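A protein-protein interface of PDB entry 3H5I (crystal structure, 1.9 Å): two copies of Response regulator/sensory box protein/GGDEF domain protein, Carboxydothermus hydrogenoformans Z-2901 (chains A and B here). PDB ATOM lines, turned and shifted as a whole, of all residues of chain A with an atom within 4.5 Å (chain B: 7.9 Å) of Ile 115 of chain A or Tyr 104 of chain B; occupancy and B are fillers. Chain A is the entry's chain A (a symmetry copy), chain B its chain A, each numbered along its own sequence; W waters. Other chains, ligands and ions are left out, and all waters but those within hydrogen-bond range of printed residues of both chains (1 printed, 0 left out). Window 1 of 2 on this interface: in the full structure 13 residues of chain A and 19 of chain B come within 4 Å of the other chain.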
ATOM      1  N   ILE A  24       7.766   1.079 -12.655  1.00  0.00           N
ATOM      2  CA  ILE A  24       8.941   1.799 -13.163  1.00  0.00           C
ATOM      3  C   ILE A  24       8.925   1.765 -14.691  1.00  0.00           C
ATOM      4  O   ILE A  24       9.088   2.804 -15.332  1.00  0.00           O
ATOM      5  CB  ILE A  24      10.288   1.221 -12.652  1.00  0.00           C
ATOM      6  CG1 ILE A  24      10.437   1.416 -11.137  1.00  0.00           C
ATOM      7  CG2 ILE A  24      11.475   1.829 -13.443  1.00  0.00           C
ATOM      8  CD1 ILE A  24      11.512   0.592 -10.472  1.00  0.00           C
ATOM      9  N   LEU A  25       8.718   0.579 -15.267  1.00  0.00           N
ATOM     10  CA  LEU A  25       8.714   0.418 -16.720  1.00  0.00           C
ATOM     11  C   LEU A  25       7.574   1.198 -17.403  1.00  0.00           C
ATOM     12  O   LEU A  25       7.777   1.791 -18.452  1.00  0.00           O
ATOM     13  CB  LEU A  25       8.640  -1.059 -17.116  1.00  0.00           C
ATOM     14  CG  LEU A  25       9.866  -1.888 -16.719  1.00  0.00           C
ATOM     15  CD1 LEU A  25       9.535  -3.355 -16.915  1.00  0.00           C
ATOM     16  CD2 LEU A  25      11.105  -1.485 -17.525  1.00  0.00           C
ATOM     17  N   TYR A  28       8.211   4.793 -18.174  1.00  0.00           N
ATOM     18  CA  TYR A  28       9.004   5.082 -19.375  1.00  0.00           C
ATOM     19  C   TYR A  28       8.322   4.671 -20.683  1.00  0.00           C
ATOM     20  O   TYR A  28       8.928   4.745 -21.754  1.00  0.00           O
ATOM     21  CB  TYR A  28      10.401   4.488 -19.215  1.00  0.00           C
ATOM     22  CG  TYR A  28      11.168   5.065 -18.052  1.00  0.00           C
ATOM     23  CD1 TYR A  28      12.038   6.146 -18.226  1.00  0.00           C
ATOM     24  CD2 TYR A  28      11.013   4.577 -16.759  1.00  0.00           C
ATOM     25  CE1 TYR A  28      12.746   6.699 -17.168  1.00  0.00           C
ATOM     26  CE2 TYR A  28      11.715   5.136 -15.677  1.00  0.00           C
ATOM     27  CZ  TYR A  28      12.589   6.203 -15.891  1.00  0.00           C
ATOM     28  OH  TYR A  28      13.306   6.758 -14.849  1.00  0.00           O
ATOM     29  N   GLU A 111      16.427   3.076 -10.532  1.00  0.00           N
ATOM     30  CA  GLU A 111      15.688   3.229 -11.789  1.00  0.00           C
ATOM     31  C   GLU A 111      16.619   3.431 -12.975  1.00  0.00           C
ATOM     32  O   GLU A 111      16.367   2.901 -14.043  1.00  0.00           O
ATOM     33  CB  GLU A 111      14.739   4.434 -11.753  1.00  0.00           C
ATOM     34  CG  GLU A 111      13.436   4.227 -11.026  1.00  0.00           C
ATOM     35  CD  GLU A 111      12.371   5.311 -11.306  1.00  0.00           C
ATOM     36  OE1 GLU A 111      12.496   6.136 -12.252  1.00  0.00           O
ATOM     37  OE2 GLU A 111      11.361   5.313 -10.563  1.00  0.00           O
ATOM     38  N   GLN A 112      17.685   4.208 -12.782  1.00  0.00           N
ATOM     39  CA  GLN A 112      18.563   4.598 -13.877  1.00  0.00           C
ATOM     40  C   GLN A 112      19.308   3.397 -14.402  1.00  0.00           C
ATOM     41  O   GLN A 112      19.462   3.228 -15.599  1.00  0.00           O
ATOM     42  CB  GLN A 112      19.578   5.659 -13.429  1.00  0.00           C
ATOM     43  CG  GLN A 112      18.969   7.018 -13.167  1.00  0.00           C
ATOM     44  CD  GLN A 112      18.473   7.234 -11.739  1.00  0.00           C
ATOM     45  OE1 GLN A 112      18.414   6.303 -10.920  1.00  0.00           O
ATOM     46  NE2 GLN A 112      18.152   8.496 -11.423  1.00  0.00           N
ATOM     47  N   VAL A 113      19.802   2.573 -13.488  1.00  0.00           N
ATOM     48  CA  VAL A 113      20.516   1.367 -13.883  1.00  0.00           C
ATOM     49  C   VAL A 113      19.548   0.395 -14.566  1.00  0.00           C
ATOM     50  O   VAL A 113      19.900  -0.195 -15.606  1.00  0.00           O
ATOM     51  CB  VAL A 113      21.253   0.708 -12.705  1.00  0.00           C
ATOM     52  CG1 VAL A 113      21.632  -0.714 -13.050  1.00  0.00           C
ATOM     53  CG2 VAL A 113      22.505   1.555 -12.359  1.00  0.00           C
ATOM     54  N   LEU A 114      18.350   0.232 -14.015  1.00  0.00           N
ATOM     55  CA  LEU A 114      17.376  -0.719 -14.588  1.00  0.00           C
ATOM     56  C   LEU A 114      16.915  -0.310 -15.978  1.00  0.00           C
ATOM     57  O   LEU A 114      16.952  -1.101 -16.901  1.00  0.00           O
ATOM     58  CB  LEU A 114      16.140  -0.896 -13.688  1.00  0.00           C
ATOM     59  CG  LEU A 114      14.981  -1.755 -14.269  1.00  0.00           C
ATOM     60  CD1 LEU A 114      15.368  -3.231 -14.399  1.00  0.00           C
ATOM     61  CD2 LEU A 114      13.734  -1.611 -13.442  1.00  0.00           C
ATOM     62  N   ILE A 115      16.509   0.944 -16.141  1.00  0.00           N
ATOM     63  CA  ILE A 115      16.015   1.385 -17.445  1.00  0.00           C
ATOM     64  C   ILE A 115      17.139   1.418 -18.467  1.00  0.00           C
ATOM     65  O   ILE A 115      16.908   1.111 -19.609  1.00  0.00           O
ATOM     66  CB  ILE A 115      15.304   2.740 -17.398  1.00  0.00           C
ATOM     67  CG1 ILE A 115      14.032   2.613 -16.574  1.00  0.00           C
ATOM     68  CG2 ILE A 115      14.893   3.176 -18.807  1.00  0.00           C
ATOM     69  CD1 ILE A 115      12.895   1.832 -17.316  1.00  0.00           C
ATOM     70  N   THR A 116      18.367   1.738 -18.055  1.00  0.00           N
ATOM     71  CA  THR A 116      19.479   1.746 -19.006  1.00  0.00           C
ATOM     72  C   THR A 116      19.749   0.342 -19.578  1.00  0.00           C
ATOM     73  O   THR A 116      19.971   0.187 -20.773  1.00  0.00           O
ATOM     74  CB  THR A 116      20.789   2.354 -18.398  1.00  0.00           C
ATOM     75  OG1 THR A 116      20.552   3.720 -18.055  1.00  0.00           O
ATOM     76  CG2 THR A 116      21.950   2.293 -19.388  1.00  0.00           C
ATOM     77  N   ILE A 117      19.713  -0.673 -18.713  1.00  0.00           N
ATOM     78  CA  ILE A 117      19.932  -2.027 -19.137  1.00  0.00           C
ATOM     79  C   ILE A 117      18.839  -2.487 -20.071  1.00  0.00           C
ATOM     80  O   ILE A 117      19.140  -3.145 -21.090  1.00  0.00           O
ATOM     81  CB  ILE A 117      20.088  -3.044 -17.955  1.00  0.00           C
ATOM     82  CG1 ILE A 117      21.319  -2.728 -17.115  1.00  0.00           C
ATOM     83  CG2 ILE A 117      20.235  -4.440 -18.536  1.00  0.00           C
ATOM     84  CD1 ILE A 117      22.606  -2.492 -17.926  1.00  0.00           C
ATOM     85  N   VAL A 118      17.594  -2.175 -19.727  1.00  0.00           N
ATOM     86  CA  VAL A 118      16.459  -2.477 -20.601  1.00  0.00           C
ATOM     87  C   VAL A 118      16.648  -1.816 -22.002  1.00  0.00           C
ATOM     88  O   VAL A 118      16.584  -2.496 -23.023  1.00  0.00           O
ATOM     89  CB  VAL A 118      15.143  -2.080 -19.915  1.00  0.00           C
ATOM     90  CG1 VAL A 118      13.965  -2.150 -20.883  1.00  0.00           C
ATOM     91  CG2 VAL A 118      14.890  -2.983 -18.688  1.00  0.00           C
ATOM     92  N   GLU A 119      16.958  -0.534 -22.020  1.00  0.00           N
ATOM     93  CA  GLU A 119      17.050   0.220 -23.286  1.00  0.00           C
ATOM     94  C   GLU A 119      18.185  -0.312 -24.119  1.00  0.00           C
ATOM     95  O   GLU A 119      18.028  -0.487 -25.295  1.00  0.00           O
ATOM     96  CB  GLU A 119      17.285   1.712 -23.031  1.00  0.00           C
ATOM     97  CG  GLU A 119      16.130   2.432 -22.331  1.00  0.00           C
ATOM     98  CD  GLU A 119      14.978   2.730 -23.257  1.00  0.00           C
ATOM     99  OE1 GLU A 119      15.148   2.589 -24.499  1.00  0.00           O
ATOM    100  OE2 GLU A 119      13.908   3.074 -22.739  1.00  0.00           O
ATOM    101  N   MET B  56      21.884  14.888 -21.957  1.00  0.00           N
ATOM    102  CA  MET B  56      20.773  15.802 -21.741  1.00  0.00           C
ATOM    103  C   MET B  56      20.260  15.755 -20.294  1.00  0.00           C
ATOM    104  O   MET B  56      19.696  14.763 -19.870  1.00  0.00           O
ATOM    105  CB  MET B  56      19.613  15.425 -22.672  1.00  0.00           C
ATOM    106  CG  MET B  56      18.401  16.356 -22.627  1.00  0.00           C
ATOM    107  SD  MET B  56      18.597  17.835 -23.663  1.00  0.00           S
ATOM    108  CE  MET B  56      18.575  17.038 -25.194  1.00  0.00           C
ATOM    109  N   ILE B  58      17.624  16.090 -17.660  1.00  0.00           N
ATOM    110  CA  ILE B  58      16.175  15.887 -17.718  1.00  0.00           C
ATOM    111  C   ILE B  58      15.371  17.148 -17.380  1.00  0.00           C
ATOM    112  O   ILE B  58      14.409  17.468 -18.071  1.00  0.00           O
ATOM    113  CB  ILE B  58      15.733  14.767 -16.751  1.00  0.00           C
ATOM    114  CG1 ILE B  58      16.105  13.410 -17.335  1.00  0.00           C
ATOM    115  CG2 ILE B  58      14.216  14.826 -16.503  1.00  0.00           C
ATOM    116  CD1 ILE B  58      15.831  12.264 -16.405  1.00  0.00           C
ATOM    117  N   VAL B  67      13.244  16.363 -21.959  1.00  0.00           N
ATOM    118  CA  VAL B  67      12.451  15.427 -22.746  1.00  0.00           C
ATOM    119  C   VAL B  67      11.912  16.152 -23.981  1.00  0.00           C
ATOM    120  O   VAL B  67      11.974  15.623 -25.068  1.00  0.00           O
ATOM    121  CB  VAL B  67      11.331  14.762 -21.912  1.00  0.00           C
ATOM    122  CG1 VAL B  67      10.402  13.930 -22.816  1.00  0.00           C
ATOM    123  CG2 VAL B  67      11.983  13.895 -20.804  1.00  0.00           C
ATOM    124  N   VAL B  81      20.542  10.043 -27.511  1.00  0.00           N
ATOM    125  CA  VAL B  81      20.444  10.860 -26.293  1.00  0.00           C
ATOM    126  C   VAL B  81      20.600   9.962 -25.057  1.00  0.00           C
ATOM    127  O   VAL B  81      19.961   8.895 -24.956  1.00  0.00           O
ATOM    128  CB  VAL B  81      19.117  11.601 -26.248  1.00  0.00           C
ATOM    129  CG1 VAL B  81      18.989  12.426 -24.942  1.00  0.00           C
ATOM    130  CG2 VAL B  81      18.968  12.530 -27.525  1.00  0.00           C
ATOM    131  N   VAL B  82      21.478  10.377 -24.157  1.00  0.00           N
ATOM    132  CA  VAL B  82      21.610   9.786 -22.827  1.00  0.00           C
ATOM    133  C   VAL B  82      21.176  10.907 -21.875  1.00  0.00           C
ATOM    134  O   VAL B  82      21.673  12.051 -21.958  1.00  0.00           O
ATOM    135  CB  VAL B  82      23.061   9.327 -22.539  1.00  0.00           C
ATOM    136  CG1 VAL B  82      23.322   8.976 -21.029  1.00  0.00           C
ATOM    137  CG2 VAL B  82      23.452   8.101 -23.435  1.00  0.00           C
ATOM    138  N   PHE B  83      20.225  10.593 -21.018  1.00  0.00           N
ATOM    139  CA  PHE B  83      19.763  11.571 -20.060  1.00  0.00           C
ATOM    140  C   PHE B  83      20.622  11.570 -18.774  1.00  0.00           C
ATOM    141  O   PHE B  83      20.961  10.529 -18.229  1.00  0.00           O
ATOM    142  CB  PHE B  83      18.326  11.306 -19.701  1.00  0.00           C
ATOM    143  CG  PHE B  83      17.371  11.640 -20.772  1.00  0.00           C
ATOM    144  CD1 PHE B  83      17.088  12.966 -21.063  1.00  0.00           C
ATOM    145  CD2 PHE B  83      16.743  10.637 -21.503  1.00  0.00           C
ATOM    146  CE1 PHE B  83      16.191  13.309 -22.057  1.00  0.00           C
ATOM    147  CE2 PHE B  83      15.845  10.993 -22.502  1.00  0.00           C
ATOM    148  CZ  PHE B  83      15.582  12.328 -22.778  1.00  0.00           C
ATOM    149  N   LEU B  84      20.875  12.778 -18.279  1.00  0.00           N
ATOM    150  CA  LEU B  84      21.468  13.033 -16.980  1.00  0.00           C
ATOM    151  C   LEU B  84      20.370  13.282 -15.955  1.00  0.00           C
ATOM    152  O   LEU B  84      19.397  14.058 -16.212  1.00  0.00           O
ATOM    153  CB  LEU B  84      22.336  14.278 -17.069  1.00  0.00           C
ATOM    154  CG  LEU B  84      23.400  14.230 -18.145  1.00  0.00           C
ATOM    155  CD1 LEU B  84      23.999  15.623 -18.431  1.00  0.00           C
ATOM    156  CD2 LEU B  84      24.456  13.176 -17.710  1.00  0.00           C
ATOM    157  N   THR B  85      20.506  12.662 -14.790  1.00  0.00           N
ATOM    158  CA  THR B  85      19.493  12.841 -13.743  1.00  0.00           C
ATOM    159  C   THR B  85      20.133  13.356 -12.442  1.00  0.00           C
ATOM    160  O   THR B  85      21.293  13.065 -12.149  1.00  0.00           O
ATOM    161  CB  THR B  85      18.673  11.551 -13.505  1.00  0.00           C
ATOM    162  OG1 THR B  85      19.494  10.559 -12.868  1.00  0.00           O
ATOM    163  CG2 THR B  85      18.141  11.015 -14.825  1.00  0.00           C
ATOM    164  N   PRO B  90      13.666  10.433 -10.994  1.00  0.00           N
ATOM    165  CA  PRO B  90      13.369  11.674 -11.723  1.00  0.00           C
ATOM    166  C   PRO B  90      11.900  11.858 -12.119  1.00  0.00           C
ATOM    167  O   PRO B  90      11.215  10.885 -12.443  1.00  0.00           O
ATOM    168  CB  PRO B  90      14.188  11.517 -13.014  1.00  0.00           C
ATOM    169  CG  PRO B  90      14.288  10.073 -13.226  1.00  0.00           C
ATOM    170  CD  PRO B  90      14.414   9.484 -11.851  1.00  0.00           C
ATOM    171  N   VAL B  92       9.788  12.208 -14.807  1.00  0.00           N
ATOM    172  CA  VAL B  92       9.825  11.930 -16.234  1.00  0.00           C
ATOM    173  C   VAL B  92       8.418  12.144 -16.732  1.00  0.00           C
ATOM    174  O   VAL B  92       7.487  11.465 -16.305  1.00  0.00           O
ATOM    175  CB  VAL B  92      10.256  10.469 -16.552  1.00  0.00           C
ATOM    176  CG1 VAL B  92      10.336  10.263 -18.048  1.00  0.00           C
ATOM    177  CG2 VAL B  92      11.586  10.155 -15.916  1.00  0.00           C
ATOM    178  N   VAL B  93       8.269  13.105 -17.636  1.00  0.00           N
ATOM    179  CA  VAL B  93       6.982  13.405 -18.213  1.00  0.00           C
ATOM    180  C   VAL B  93       6.536  12.254 -19.126  1.00  0.00           C
ATOM    181  O   VAL B  93       7.358  11.480 -19.648  1.00  0.00           O
ATOM    182  CB  VAL B  93       7.004  14.771 -18.953  1.00  0.00           C
ATOM    183  CG1 VAL B  93       7.303  15.903 -17.942  1.00  0.00           C
ATOM    184  CG2 VAL B  93       8.021  14.757 -20.101  1.00  0.00           C
ATOM    185  N   ILE B  96       8.114  11.067 -22.526  1.00  0.00           N
ATOM    186  CA  ILE B  96       9.285  10.175 -22.627  1.00  0.00           C
ATOM    187  C   ILE B  96       9.002   8.957 -23.516  1.00  0.00           C
ATOM    188  O   ILE B  96       9.921   8.439 -24.173  1.00  0.00           O
ATOM    189  CB  ILE B  96       9.765   9.711 -21.213  1.00  0.00           C
ATOM    190  CG1 ILE B  96      11.155   9.057 -21.286  1.00  0.00           C
ATOM    191  CG2 ILE B  96       8.713   8.775 -20.572  1.00  0.00           C
ATOM    192  CD1 ILE B  96      12.253   9.983 -21.734  1.00  0.00           C
ATOM    193  N   ARG B  97       7.738   8.532 -23.560  1.00  0.00           N
ATOM    194  CA  ARG B  97       7.284   7.437 -24.427  1.00  0.00           C
ATOM    195  C   ARG B  97       7.608   7.649 -25.917  1.00  0.00           C
ATOM    196  O   ARG B  97       7.699   6.675 -26.659  1.00  0.00           O
ATOM    197  CB  ARG B  97       5.771   7.207 -24.272  1.00  0.00           C
ATOM    198  CG  ARG B  97       4.900   8.308 -24.944  1.00  0.00           C
ATOM    199  CD  ARG B  97       3.420   7.958 -25.143  1.00  0.00           C
ATOM    200  NE  ARG B  97       2.729   7.659 -23.882  1.00  0.00           N
ATOM    201  CZ  ARG B  97       1.414   7.782 -23.680  1.00  0.00           C
ATOM    202  NH1 ARG B  97       0.617   8.226 -24.648  1.00  0.00           N
ATOM    203  NH2 ARG B  97       0.895   7.469 -22.488  1.00  0.00           N
ATOM    204  N   VAL B  99      10.374   9.428 -27.035  1.00  0.00           N
ATOM    205  CA  VAL B  99      11.798   9.748 -27.173  1.00  0.00           C
ATOM    206  C   VAL B  99      12.601   8.460 -27.203  1.00  0.00           C
ATOM    207  O   VAL B  99      12.344   7.584 -26.396  1.00  0.00           O
ATOM    208  CB  VAL B  99      12.237  10.646 -25.986  1.00  0.00           C
ATOM    209  CG1 VAL B  99      13.757  10.808 -25.939  1.00  0.00           C
ATOM    210  CG2 VAL B  99      11.524  11.981 -26.086  1.00  0.00           C
ATOM    211  N   THR B 100      13.557   8.331 -28.127  1.00  0.00           N
ATOM    212  CA  THR B 100      14.480   7.178 -28.105  1.00  0.00           C
ATOM    213  C   THR B 100      15.642   7.537 -27.179  1.00  0.00           C
ATOM    214  O   THR B 100      16.403   8.474 -27.462  1.00  0.00           O
ATOM    215  CB  THR B 100      15.030   6.826 -29.515  1.00  0.00           C
ATOM    216  OG1 THR B 100      13.952   6.839 -30.445  1.00  0.00           O
ATOM    217  CG2 THR B 100      15.673   5.453 -29.532  1.00  0.00           C
ATOM    218  N   ALA B 101      15.701   6.874 -26.030  1.00  0.00           N
ATOM    219  CA  ALA B 101      16.764   7.090 -25.048  1.00  0.00           C
ATOM    220  C   ALA B 101      17.762   5.933 -25.131  1.00  0.00           C
ATOM    221  O   ALA B 101      17.364   4.787 -25.302  1.00  0.00           O
ATOM    222  CB  ALA B 101      16.172   7.177 -23.647  1.00  0.00           C
ATOM    223  N   TYR B 102      19.039   6.227 -25.032  1.00  0.00           N
ATOM    224  CA  TYR B 102      20.067   5.202 -25.000  1.00  0.00           C
ATOM    225  C   TYR B 102      20.543   4.904 -23.579  1.00  0.00           C
ATOM    226  O   TYR B 102      21.303   3.963 -23.368  1.00  0.00           O
ATOM    227  CB  TYR B 102      21.267   5.594 -25.841  1.00  0.00           C
ATOM    228  CG  TYR B 102      21.063   5.348 -27.317  1.00  0.00           C
ATOM    229  CD1 TYR B 102      20.089   6.054 -28.034  1.00  0.00           C
ATOM    230  CD2 TYR B 102      21.807   4.376 -27.978  1.00  0.00           C
ATOM    231  CE1 TYR B 102      19.880   5.818 -29.390  1.00  0.00           C
ATOM    232  CE2 TYR B 102      21.610   4.136 -29.334  1.00  0.00           C
ATOM    233  CZ  TYR B 102      20.654   4.859 -30.032  1.00  0.00           C
ATOM    234  OH  TYR B 102      20.487   4.602 -31.375  1.00  0.00           O
ATOM    235  N   GLY B 103      20.142   5.729 -22.610  1.00  0.00           N
ATOM    236  CA  GLY B 103      20.599   5.509 -21.268  1.00  0.00           C
ATOM    237  C   GLY B 103      20.177   6.634 -20.352  1.00  0.00           C
ATOM    238  O   GLY B 103      19.712   7.669 -20.821  1.00  0.00           O
ATOM    239  N   TYR B 104      20.344   6.388 -19.057  1.00  0.00           N
ATOM    240  CA  TYR B 104      20.132   7.395 -17.997  1.00  0.00           C
ATOM    241  C   TYR B 104      21.281   7.249 -17.040  1.00  0.00           C
ATOM    242  O   TYR B 104      21.575   6.131 -16.584  1.00  0.00           O
ATOM    243  CB  TYR B 104      18.832   7.146 -17.216  1.00  0.00           C
ATOM    244  CG  TYR B 104      17.586   7.297 -18.057  1.00  0.00           C
ATOM    245  CD1 TYR B 104      16.824   8.445 -18.001  1.00  0.00           C
ATOM    246  CD2 TYR B 104      17.191   6.281 -18.920  1.00  0.00           C
ATOM    247  CE1 TYR B 104      15.677   8.589 -18.795  1.00  0.00           C
ATOM    248  CE2 TYR B 104      16.057   6.424 -19.723  1.00  0.00           C
ATOM    249  CZ  TYR B 104      15.311   7.576 -19.638  1.00  0.00           C
ATOM    250  OH  TYR B 104      14.195   7.700 -20.420  1.00  0.00           O
ATOM    251  N   VAL B 105      21.894   8.357 -16.666  1.00  0.00           N
ATOM    252  CA  VAL B 105      22.974   8.317 -15.715  1.00  0.00           C
ATOM    253  C   VAL B 105      22.838   9.449 -14.696  1.00  0.00           C
ATOM    254  O   VAL B 105      22.436  10.568 -15.042  1.00  0.00           O
ATOM    255  CB  VAL B 105      24.326   8.332 -16.432  1.00  0.00           C
ATOM    256  CG1 VAL B 105      24.472   9.535 -17.312  1.00  0.00           C
ATOM    257  CG2 VAL B 105      25.470   8.230 -15.452  1.00  0.00           C
ATOM    258  N   MET B 106      23.122   9.121 -13.442  1.00  0.00           N
ATOM    259  CA  MET B 106      23.151  10.110 -12.360  1.00  0.00           C
ATOM    260  C   MET B 106      24.304  11.097 -12.562  1.00  0.00           C
ATOM    261  O   MET B 106      25.436  10.704 -12.884  1.00  0.00           O
ATOM    262  CB  MET B 106      23.282   9.423 -10.991  1.00  0.00           C
ATOM    263  CG  MET B 106      22.039   8.618 -10.551  1.00  0.00           C
ATOM    264  SD  MET B 106      22.156   8.024  -8.816  1.00  0.00           S
ATOM    265  CE  MET B 106      23.708   7.127  -8.826  1.00  0.00           C
ATOM    266  N   LYS B 107      24.047  12.386 -12.355  1.00  0.00           N
ATOM    267  CA  LYS B 107      25.135  13.368 -12.435  1.00  0.00           C
ATOM    268  C   LYS B 107      26.220  13.120 -11.351  1.00  0.00           C
ATOM    269  O   LYS B 107      27.369  13.488 -11.529  1.00  0.00           O
ATOM    270  CB  LYS B 107      24.581  14.799 -12.388  1.00  0.00           C
ATOM    271  CG  LYS B 107      24.116  15.251 -13.782  1.00  0.00           C
ATOM    272  CD  LYS B 107      23.503  16.631 -13.800  1.00  0.00           C
ATOM    273  CE  LYS B 107      22.117  16.622 -13.243  1.00  0.00           C
ATOM    274  NZ  LYS B 107      21.502  17.954 -13.386  1.00  0.00           N
ATOM    275  N   ALA B 109      27.285  10.067 -10.706  1.00  0.00           N
ATOM    276  CA  ALA B 109      27.905   8.767 -11.025  1.00  0.00           C
ATOM    277  C   ALA B 109      29.418   8.885 -11.235  1.00  0.00           C
ATOM    278  O   ALA B 109      29.954   9.936 -11.618  1.00  0.00           O
ATOM    279  CB  ALA B 109      27.245   8.120 -12.270  1.00  0.00           C
ATOM    280  N   VAL B 113      31.196   4.684 -14.849  1.00  0.00           N
ATOM    281  CA  VAL B 113      29.819   4.487 -15.278  1.00  0.00           C
ATOM    282  C   VAL B 113      29.485   5.467 -16.408  1.00  0.00           C
ATOM    283  O   VAL B 113      28.854   5.065 -17.404  1.00  0.00           O
ATOM    284  CB  VAL B 113      28.821   4.595 -14.112  1.00  0.00           C
ATOM    285  CG1 VAL B 113      27.417   4.787 -14.638  1.00  0.00           C
ATOM    286  CG2 VAL B 113      28.925   3.316 -13.242  1.00  0.00           C
ATOM    287  N   ILE B 117      28.698   4.314 -20.459  1.00  0.00           N
ATOM    288  CA  ILE B 117      27.435   4.580 -21.089  1.00  0.00           C
ATOM    289  C   ILE B 117      27.621   5.345 -22.376  1.00  0.00           C
ATOM    290  O   ILE B 117      26.957   5.022 -23.384  1.00  0.00           O
ATOM    291  CB  ILE B 117      26.411   5.324 -20.167  1.00  0.00           C
ATOM    292  CG1 ILE B 117      26.037   4.474 -18.959  1.00  0.00           C
ATOM    293  CG2 ILE B 117      25.156   5.611 -20.973  1.00  0.00           C
ATOM    294  CD1 ILE B 117      25.655   3.021 -19.291  1.00  0.00           C
HETATM  295  O   HOH W   1      21.561   5.408 -10.271  1.00  0.00           O
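OG1 of Thr 85 of chain B sits at hydrogen-bond distance from NE2 of Gln 112 of chain A. The backbone NH (N) of Tyr 104 of chain B is in hydrogen-bond range of the side-chain hydroxyl (OG1) of Thr 116 of chain A (2.9 Å). O of Ala 101 of chain B sits close to OE1 of Glu 119 of chain A, 3.2 Å away.
O of Gly 103 of chain B is in hydrogen-bond range of N of Phe 83 of chain B (3.0 Å). N of Thr 85 of chain B is in hydrogen-bond range of O of Val 105 of chain B. The backbone NH of Lys 107 of chain B is in hydrogen-bond range of the backbone carbonyl oxygen of Thr 85 of chain B (2.8 Å). OE1 of Glu 111 of chain A is in hydrogen-bond range of OH of Tyr 28 of chain A, 2.8 Å away. O of Gln 112 of chain A lies within hydrogen-bond range of OG1 of Thr 116 of chain A.
Among the printed residues, pairs that only touch across the chains: Tyr 28 of chain A with Pro 90 of chain B (3.8 Å), Tyr 28 of chain A with Val 92 of chain B (3.9 Å), Tyr 28 of chain A with Ile 96 of chain B (3.9 Å), Tyr 28 of chain A with Tyr 104 of chain B (3.4 Å), Glu 111 of chain A with Pro 90 of chain B (3.9 Å), Gln 112 of chain A with Pro 90 of chain B (3.9 Å), Gln 112 of chain A with Tyr 104 of chain B (3.7 Å), Gln 112 of chain A with Met 106 of chain B (3.99 Å), Ile 115 of chain A with Tyr 104 of chain B (3.6 Å), Thr 116 of chain A with Gly 103 of chain B (3.7 Å) and Thr 116 of chain A with Ile 117 of chain B (3.8 Å).
Of chain B, only Tyr 104 (3.6 Å) comes within 4 Å of Ile 115 of chain A. Printed residues of chain A within 4 Å of Val 92 of chain B: Tyr 28 (3.9 Å). Of the printed residues of chain A, Ile 96 of chain B touches Tyr 28. Of the printed residues of chain A, Thr 85 of chain B touches Gln 112. Printed residues of chain A within 4 Å of Ala 101 of chain B: Glu 119. Printed residues of chain A within 4 Å of Pro 90 of chain B: Tyr 28, Glu 111 and Gln 112. The nearest printed residue of chain A that does not touch Ile 117 of chain B is Ile 117 of chain A (6.4 Å).
Hydrophobic or aromatic side chains of chain A within 4 Å of the printed part of chain B: Tyr 28 and Ile 115. Among the printed residues, 14 pairs touch across the chains.
2 positions are printed for both chains.
Water W1 lies within hydrogen-bond range of SD of Met 106 of chain B and OE1 of Gln 112 of chain A.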
